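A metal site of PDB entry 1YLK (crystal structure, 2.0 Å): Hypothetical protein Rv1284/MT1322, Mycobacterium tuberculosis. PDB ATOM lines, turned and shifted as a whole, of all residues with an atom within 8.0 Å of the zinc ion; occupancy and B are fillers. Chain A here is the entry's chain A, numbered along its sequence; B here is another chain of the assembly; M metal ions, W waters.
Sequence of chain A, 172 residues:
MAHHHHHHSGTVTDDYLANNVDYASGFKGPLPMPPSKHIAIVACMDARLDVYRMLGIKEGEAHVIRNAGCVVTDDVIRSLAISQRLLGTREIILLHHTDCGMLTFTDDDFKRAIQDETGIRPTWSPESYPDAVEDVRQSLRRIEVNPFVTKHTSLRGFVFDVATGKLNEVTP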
ATOM      1  N   ALA A  43     -11.250  13.713 -14.914  1.00  0.00           N
ATOM      2  CA  ALA A  43     -10.946  15.125 -14.819  1.00  0.00           C
ATOM      3  C   ALA A  43     -12.160  15.961 -15.219  1.00  0.00           C
ATOM      4  O   ALA A  43     -13.112  15.434 -15.817  1.00  0.00           O
ATOM      5  CB  ALA A  43      -9.743  15.466 -15.698  1.00  0.00           C
ATOM      6  N   CYS A  44     -12.156  17.254 -14.869  1.00  0.00           N
ATOM      7  CA  CYS A  44     -13.215  18.150 -15.367  1.00  0.00           C
ATOM      8  C   CYS A  44     -12.958  18.402 -16.838  1.00  0.00           C
ATOM      9  O   CYS A  44     -11.816  18.356 -17.287  1.00  0.00           O
ATOM     10  CB  CYS A  44     -13.185  19.510 -14.648  1.00  0.00           C
ATOM     11  SG  CYS A  44     -14.542  20.617 -15.148  1.00  0.00           S
ATOM     12  N   MET A  45     -14.025  18.728 -17.567  1.00  0.00           N
ATOM     13  CA  MET A  45     -13.950  19.098 -18.980  1.00  0.00           C
ATOM     14  C   MET A  45     -13.361  20.503 -19.189  1.00  0.00           C
ATOM     15  O   MET A  45     -13.121  20.899 -20.325  1.00  0.00           O
ATOM     16  CB  MET A  45     -15.338  19.070 -19.596  1.00  0.00           C
ATOM     17  CG  MET A  45     -16.246  20.224 -19.152  1.00  0.00           C
ATOM     18  SD  MET A  45     -17.884  20.086 -19.874  1.00  0.00           S
ATOM     19  CE  MET A  45     -18.741  21.527 -19.251  1.00  0.00           C
ATOM     20  N   ASP A  46     -13.138  21.226 -18.099  1.00  0.00           N
ATOM     21  CA  ASP A  46     -12.650  22.606 -18.120  1.00  0.00           C
ATOM     22  C   ASP A  46     -11.587  22.876 -19.199  1.00  0.00           C
ATOM     23  O   ASP A  46     -10.605  22.119 -19.352  1.00  0.00           O
ATOM     24  CB  ASP A  46     -12.120  23.014 -16.730  1.00  0.00           C
ATOM     25  CG  ASP A  46     -11.929  24.526 -16.591  1.00  0.00           C
ATOM     26  OD1 ASP A  46     -10.936  25.038 -17.108  1.00  0.00           O
ATOM     27  OD2 ASP A  46     -12.769  25.200 -15.976  1.00  0.00           O
ATOM     28  N   ALA A  47     -11.786  23.981 -19.914  1.00  0.00           N
ATOM     29  CA  ALA A  47     -10.949  24.386 -21.029  1.00  0.00           C
ATOM     30  C   ALA A  47      -9.489  24.677 -20.645  1.00  0.00           C
ATOM     31  O   ALA A  47      -8.602  24.662 -21.518  1.00  0.00           O
ATOM     32  CB  ALA A  47     -11.567  25.601 -21.691  1.00  0.00           C
ATOM     33  N   ARG A  48      -9.239  24.928 -19.367  1.00  0.00           N
ATOM     34  CA  ARG A  48      -7.907  25.325 -18.914  1.00  0.00           C
ATOM     35  C   ARG A  48      -7.075  24.130 -18.445  1.00  0.00           C
ATOM     36  O   ARG A  48      -5.928  24.274 -18.046  1.00  0.00           O
ATOM     37  CB  ARG A  48      -8.022  26.377 -17.815  1.00  0.00           C
ATOM     38  CG  ARG A  48      -8.768  27.639 -18.258  1.00  0.00           C
ATOM     39  CD  ARG A  48      -9.216  28.448 -17.055  1.00  0.00           C
ATOM     40  NE  ARG A  48     -10.272  27.769 -16.309  1.00  0.00           N
ATOM     41  CZ  ARG A  48     -10.890  28.297 -15.263  1.00  0.00           C
ATOM     42  NH1 ARG A  48     -10.539  29.512 -14.828  1.00  0.00           N
ATOM     43  NH2 ARG A  48     -11.842  27.612 -14.633  1.00  0.00           N
ATOM     44  N   LEU A  49      -7.680  22.942 -18.507  1.00  0.00           N
ATOM     45  CA  LEU A  49      -6.984  21.714 -18.130  1.00  0.00           C
ATOM     46  C   LEU A  49      -6.572  20.904 -19.338  1.00  0.00           C
ATOM     47  O   LEU A  49      -7.391  20.255 -19.979  1.00  0.00           O
ATOM     48  CB  LEU A  49      -7.872  20.863 -17.205  1.00  0.00           C
ATOM     49  CG  LEU A  49      -7.911  21.197 -15.709  1.00  0.00           C
ATOM     50  CD1 LEU A  49      -8.468  22.587 -15.448  1.00  0.00           C
ATOM     51  CD2 LEU A  49      -8.756  20.124 -15.010  1.00  0.00           C
ATOM     52  N   ARG A  66     -13.525  12.563 -18.788  1.00  0.00           N
ATOM     53  CA  ARG A  66     -13.797  13.963 -18.460  1.00  0.00           C
ATOM     54  C   ARG A  66     -15.253  14.306 -18.587  1.00  0.00           C
ATOM     55  O   ARG A  66     -15.931  13.890 -19.545  1.00  0.00           O
ATOM     56  CB  ARG A  66     -12.977  14.889 -19.367  1.00  0.00           C
ATOM     57  CG  ARG A  66     -11.492  14.614 -19.362  1.00  0.00           C
ATOM     58  CD  ARG A  66     -10.743  15.641 -20.236  1.00  0.00           C
ATOM     59  NE  ARG A  66     -10.740  16.960 -19.627  1.00  0.00           N
ATOM     60  CZ  ARG A  66      -9.953  17.974 -20.003  1.00  0.00           C
ATOM     61  NH1 ARG A  66      -9.074  17.784 -20.980  1.00  0.00           N
ATOM     62  NH2 ARG A  66     -10.019  19.139 -19.373  1.00  0.00           N
ATOM     63  N   ASN A  67     -15.750  15.073 -17.610  1.00  0.00           N
ATOM     64  CA  ASN A  67     -17.107  15.607 -17.677  1.00  0.00           C
ATOM     65  C   ASN A  67     -17.214  16.934 -16.934  1.00  0.00           C
ATOM     66  O   ASN A  67     -16.225  17.416 -16.370  1.00  0.00           O
ATOM     67  CB  ASN A  67     -18.130  14.556 -17.181  1.00  0.00           C
ATOM     68  CG  ASN A  67     -17.992  14.263 -15.673  1.00  0.00           C
ATOM     69  OD1 ASN A  67     -17.388  15.016 -14.923  1.00  0.00           O
ATOM     70  ND2 ASN A  67     -18.573  13.149 -15.244  1.00  0.00           N
ATOM     71  N   ALA A  68     -18.390  17.538 -16.903  1.00  0.00           N
ATOM     72  CA  ALA A  68     -18.555  18.783 -16.157  1.00  0.00           C
ATOM     73  C   ALA A  68     -18.392  18.541 -14.649  1.00  0.00           C
ATOM     74  O   ALA A  68     -19.166  17.805 -14.051  1.00  0.00           O
ATOM     75  CB  ALA A  68     -19.939  19.396 -16.449  1.00  0.00           C
ATOM     76  N   GLY A  69     -17.355  19.151 -14.069  1.00  0.00           N
ATOM     77  CA  GLY A  69     -17.149  19.122 -12.623  1.00  0.00           C
ATOM     78  C   GLY A  69     -16.308  17.977 -12.081  1.00  0.00           C
ATOM     79  O   GLY A  69     -16.066  17.920 -10.865  1.00  0.00           O
ATOM     80  N   CYS A  70     -15.846  17.080 -12.954  1.00  0.00           N
ATOM     81  CA  CYS A  70     -15.163  15.830 -12.543  1.00  0.00           C
ATOM     82  C   CYS A  70     -16.050  15.029 -11.566  1.00  0.00           C
ATOM     83  O   CYS A  70     -15.610  14.577 -10.493  1.00  0.00           O
ATOM     84  CB  CYS A  70     -13.761  16.118 -11.959  1.00  0.00           C
ATOM     85  SG  CYS A  70     -12.754  14.626 -11.566  1.00  0.00           S
ATOM     86  N   LEU A  95      -9.125  14.481 -10.773  1.00  0.00           N
ATOM     87  CA  LEU A  95      -8.688  15.864 -10.865  1.00  0.00           C
ATOM     88  C   LEU A  95      -9.868  16.811 -10.888  1.00  0.00           C
ATOM     89  O   LEU A  95     -10.538  16.963 -11.912  1.00  0.00           O
ATOM     90  CB  LEU A  95      -7.840  16.105 -12.115  1.00  0.00           C
ATOM     91  CG  LEU A  95      -6.623  15.210 -12.355  1.00  0.00           C
ATOM     92  CD1 LEU A  95      -6.082  15.479 -13.754  1.00  0.00           C
ATOM     93  CD2 LEU A  95      -5.551  15.451 -11.317  1.00  0.00           C
ATOM     94  N   HIS A  96     -10.101  17.447  -9.741  1.00  0.00           N
ATOM     95  CA  HIS A  96     -10.929  18.633  -9.649  1.00  0.00           C
ATOM     96  C   HIS A  96      -9.992  19.812  -9.856  1.00  0.00           C
ATOM     97  O   HIS A  96      -8.798  19.637 -10.034  1.00  0.00           O
ATOM     98  CB  HIS A  96     -11.585  18.721  -8.256  1.00  0.00           C
ATOM     99  CG  HIS A  96     -12.841  17.921  -8.114  1.00  0.00           C
ATOM    100  ND1 HIS A  96     -12.958  16.619  -8.529  1.00  0.00           N
ATOM    101  CD2 HIS A  96     -14.031  18.232  -7.528  1.00  0.00           C
ATOM    102  CE1 HIS A  96     -14.168  16.167  -8.249  1.00  0.00           C
ATOM    103  NE2 HIS A  96     -14.845  17.131  -7.661  1.00  0.00           N
ATOM    104  N   HIS A  97     -10.506  21.022  -9.810  1.00  0.00           N
ATOM    105  CA  HIS A  97      -9.645  22.183  -9.968  1.00  0.00           C
ATOM    106  C   HIS A  97     -10.298  23.396  -9.335  1.00  0.00           C
ATOM    107  O   HIS A  97     -11.506  23.393  -9.105  1.00  0.00           O
ATOM    108  CB  HIS A  97      -9.393  22.439 -11.447  1.00  0.00           C
ATOM    109  CG  HIS A  97     -10.614  22.826 -12.192  1.00  0.00           C
ATOM    110  ND1 HIS A  97     -10.946  24.136 -12.432  1.00  0.00           N
ATOM    111  CD2 HIS A  97     -11.607  22.078 -12.733  1.00  0.00           C
ATOM    112  CE1 HIS A  97     -12.089  24.187 -13.100  1.00  0.00           C
ATOM    113  NE2 HIS A  97     -12.516  22.945 -13.284  1.00  0.00           N
ATOM    114  N   THR A  98      -9.485  24.418  -9.077  1.00  0.00           N
ATOM    115  CA  THR A  98      -9.948  25.701  -8.532  1.00  0.00           C
ATOM    116  C   THR A  98     -10.721  26.481  -9.612  1.00  0.00           C
ATOM    117  O   THR A  98     -10.462  26.288 -10.813  1.00  0.00           O
ATOM    118  CB  THR A  98      -8.745  26.571  -8.063  1.00  0.00           C
ATOM    119  OG1 THR A  98      -7.870  26.797  -9.169  1.00  0.00           O
ATOM    120  CG2 THR A  98      -7.953  25.880  -6.932  1.00  0.00           C
ATOM    121  N   ASP A  99     -11.637  27.357  -9.201  1.00  0.00           N
ATOM    122  CA  ASP A  99     -12.459  28.123 -10.156  1.00  0.00           C
ATOM    123  C   ASP A  99     -13.278  27.226 -11.102  1.00  0.00           C
ATOM    124  O   ASP A  99     -13.336  27.462 -12.315  1.00  0.00           O
ATOM    125  CB  ASP A  99     -11.600  29.110 -10.963  1.00  0.00           C
ATOM    126  CG  ASP A  99     -12.416  30.259 -11.582  1.00  0.00           C
ATOM    127  OD1 ASP A  99     -13.206  30.883 -10.857  1.00  0.00           O
ATOM    128  OD2 ASP A  99     -12.230  30.555 -12.780  1.00  0.00           O
ATOM    129  N   CYS A 100     -13.884  26.178 -10.557  1.00  0.00           N
ATOM    130  CA  CYS A 100     -14.682  25.278 -11.362  1.00  0.00           C
ATOM    131  C   CYS A 100     -16.052  25.875 -11.606  1.00  0.00           C
ATOM    132  O   CYS A 100     -16.638  26.467 -10.711  1.00  0.00           O
ATOM    133  CB  CYS A 100     -14.812  23.910 -10.698  1.00  0.00           C
ATOM    134  SG  CYS A 100     -15.588  22.672 -11.754  1.00  0.00           S
ATOM    135  N   GLY A 101     -16.558  25.723 -12.831  1.00  0.00           N
ATOM    136  CA  GLY A 101     -17.904  26.185 -13.177  1.00  0.00           C
ATOM    137  C   GLY A 101     -19.001  25.582 -12.313  1.00  0.00           C
ATOM    138  O   GLY A 101     -20.084  26.161 -12.184  1.00  0.00           O
ATOM    139  N   MET A 102     -18.705  24.447 -11.698  1.00  0.00           N
ATOM    140  CA  MET A 102     -19.665  23.747 -10.840  1.00  0.00           C
ATOM    141  C   MET A 102     -19.909  24.453  -9.506  1.00  0.00           C
ATOM    142  O   MET A 102     -20.887  24.140  -8.811  1.00  0.00           O
ATOM    143  CB  MET A 102     -19.228  22.298 -10.584  1.00  0.00           C
ATOM    144  CG  MET A 102     -19.092  21.446 -11.844  1.00  0.00           C
ATOM    145  SD  MET A 102     -20.480  21.452 -12.983  1.00  0.00           S
ATOM    146  CE  MET A 102     -21.689  20.597 -12.010  1.00  0.00           C
ATOM    147  N   LEU A 103     -19.034  25.390  -9.139  1.00  0.00           N
ATOM    148  CA  LEU A 103     -19.203  26.150  -7.910  1.00  0.00           C
ATOM    149  C   LEU A 103     -20.072  27.393  -8.162  1.00  0.00           C
ATOM    150  O   LEU A 103     -20.437  28.080  -7.218  1.00  0.00           O
ATOM    151  CB  LEU A 103     -17.854  26.590  -7.314  1.00  0.00           C
ATOM    152  CG  LEU A 103     -16.672  25.612  -7.167  1.00  0.00           C
ATOM    153  CD1 LEU A 103     -15.528  26.311  -6.460  1.00  0.00           C
ATOM    154  CD2 LEU A 103     -17.057  24.351  -6.408  1.00  0.00           C
ATOM    155  N   TYR A 129     -21.750  21.501  -6.941  1.00  0.00           N
ATOM    156  CA  TYR A 129     -21.198  21.357  -5.597  1.00  0.00           C
ATOM    157  C   TYR A 129     -20.518  22.659  -5.170  1.00  0.00           C
ATOM    158  O   TYR A 129     -19.959  23.352  -6.011  1.00  0.00           O
ATOM    159  CB  TYR A 129     -20.238  20.166  -5.500  1.00  0.00           C
ATOM    160  CG  TYR A 129     -19.139  20.093  -6.557  1.00  0.00           C
ATOM    161  CD1 TYR A 129     -17.933  20.772  -6.388  1.00  0.00           C
ATOM    162  CD2 TYR A 129     -19.304  19.319  -7.722  1.00  0.00           C
ATOM    163  CE1 TYR A 129     -16.914  20.692  -7.337  1.00  0.00           C
ATOM    164  CE2 TYR A 129     -18.279  19.229  -8.693  1.00  0.00           C
ATOM    165  CZ  TYR A 129     -17.082  19.931  -8.467  1.00  0.00           C
ATOM    166  OH  TYR A 129     -16.047  19.883  -9.370  1.00  0.00           O
ATOM    167  N   VAL A 162      -5.667  26.492 -11.105  1.00  0.00           N
ATOM    168  CA  VAL A 162      -5.674  27.061 -12.475  1.00  0.00           C
ATOM    169  C   VAL A 162      -4.834  28.314 -12.595  1.00  0.00           C
ATOM    170  O   VAL A 162      -4.678  28.884 -13.688  1.00  0.00           O
ATOM    171  CB  VAL A 162      -7.127  27.301 -13.021  1.00  0.00           C
ATOM    172  CG1 VAL A 162      -7.880  25.971 -13.136  1.00  0.00           C
ATOM    173  CG2 VAL A 162      -7.883  28.309 -12.181  1.00  0.00           C
ATOM    174  N   MET B  33     -12.681  31.254 -17.499  1.00  0.00           N
ATOM    175  CA  MET B  33     -13.361  29.953 -17.513  1.00  0.00           C
ATOM    176  C   MET B  33     -14.005  29.587 -18.863  1.00  0.00           C
ATOM    177  O   MET B  33     -13.909  28.437 -19.284  1.00  0.00           O
ATOM    178  CB  MET B  33     -14.424  29.925 -16.403  1.00  0.00           C
ATOM    179  CG  MET B  33     -15.024  28.559 -16.127  1.00  0.00           C
ATOM    180  SD  MET B  33     -16.445  28.747 -15.021  1.00  0.00           S
ATOM    181  CE  MET B  33     -15.731  29.559 -13.608  1.00  0.00           C
ATOM    182  N   HIS B  63     -13.814  22.901 -24.259  1.00  0.00           N
ATOM    183  CA  HIS B  63     -14.211  21.824 -23.378  1.00  0.00           C
ATOM    184  C   HIS B  63     -13.944  20.480 -24.020  1.00  0.00           C
ATOM    185  O   HIS B  63     -14.243  20.272 -25.206  1.00  0.00           O
ATOM    186  CB  HIS B  63     -15.681  21.934 -23.007  1.00  0.00           C
ATOM    187  CG  HIS B  63     -15.977  23.001 -22.010  1.00  0.00           C
ATOM    188  ND1 HIS B  63     -17.146  23.719 -22.024  1.00  0.00           N
ATOM    189  CD2 HIS B  63     -15.259  23.461 -20.961  1.00  0.00           C
ATOM    190  CE1 HIS B  63     -17.144  24.576 -21.025  1.00  0.00           C
ATOM    191  NE2 HIS B  63     -16.002  24.451 -20.371  1.00  0.00           N
ATOM    192  N   LEU B  87     -21.469  28.364 -20.065  1.00  0.00           N
ATOM    193  CA  LEU B  87     -20.136  28.758 -20.528  1.00  0.00           C
ATOM    194  C   LEU B  87     -20.057  29.089 -22.030  1.00  0.00           C
ATOM    195  O   LEU B  87     -18.967  29.261 -22.573  1.00  0.00           O
ATOM    196  CB  LEU B  87     -19.129  27.672 -20.118  1.00  0.00           C
ATOM    197  CG  LEU B  87     -18.979  27.579 -18.583  1.00  0.00           C
ATOM    198  CD1 LEU B  87     -18.355  26.273 -18.116  1.00  0.00           C
ATOM    199  CD2 LEU B  87     -18.229  28.775 -18.050  1.00  0.00           C
HETATM  200 ZN    ZN M   1     -14.434  22.457 -13.722  1.00  0.00          ZN
HETATM  201  O   HOH W   1     -14.661  24.503 -14.611  1.00  0.00           O
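CB of Asp 46 touches the zinc ion (3.8 Å).
Gly 101 touches the zinc ion.
Of the 26 residues printed, 5 come within 4 Å of the zinc ion.
Along chain A the residues within 4 Å of the zinc ion span positions 44 to 101.
The zinc ion is bound by NE2 of His 97.
Water W1 binds the zinc ion (2.2 Å).
SG of Cys 100 is bound to the zinc ion (2.3 Å).
SG of Cys 44 binds the zinc ion (2.3 Å).
The backbone carbonyl oxygen (O) of Asp 46 sits at hydrogen-bond distance from the guanidinium group (NH2) of Arg 66 (3.0 Å).
N of Met 102 sits close to SG of Cys 100 (3.6 Å).
The backbone carbonyl oxygen (O) of Leu 95 is in hydrogen-bond range of the backbone NH (N) of Cys 44, at 3.4 Å.
NH2 of Arg 48 is in salt-bridge range of OD2 of Asp 46, at 2.9 Å.
SG of Cys 44 lies close to N of Asp 46, 3.3 Å away.
The side-chain sulfur of Cys 100 sits close to the side-chain hydroxyl of Tyr 129 (3.7 Å).
SG of Cys 44 sits close to N of Gly 69, 3.4 Å away.
N of Gly 101 lies close to SD of Met 33 of chain B (3.7 Å).
Water W1 bridges OD2 of Asp 46 (2.4 Å) and N of Gly 101 (2.9 Å).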
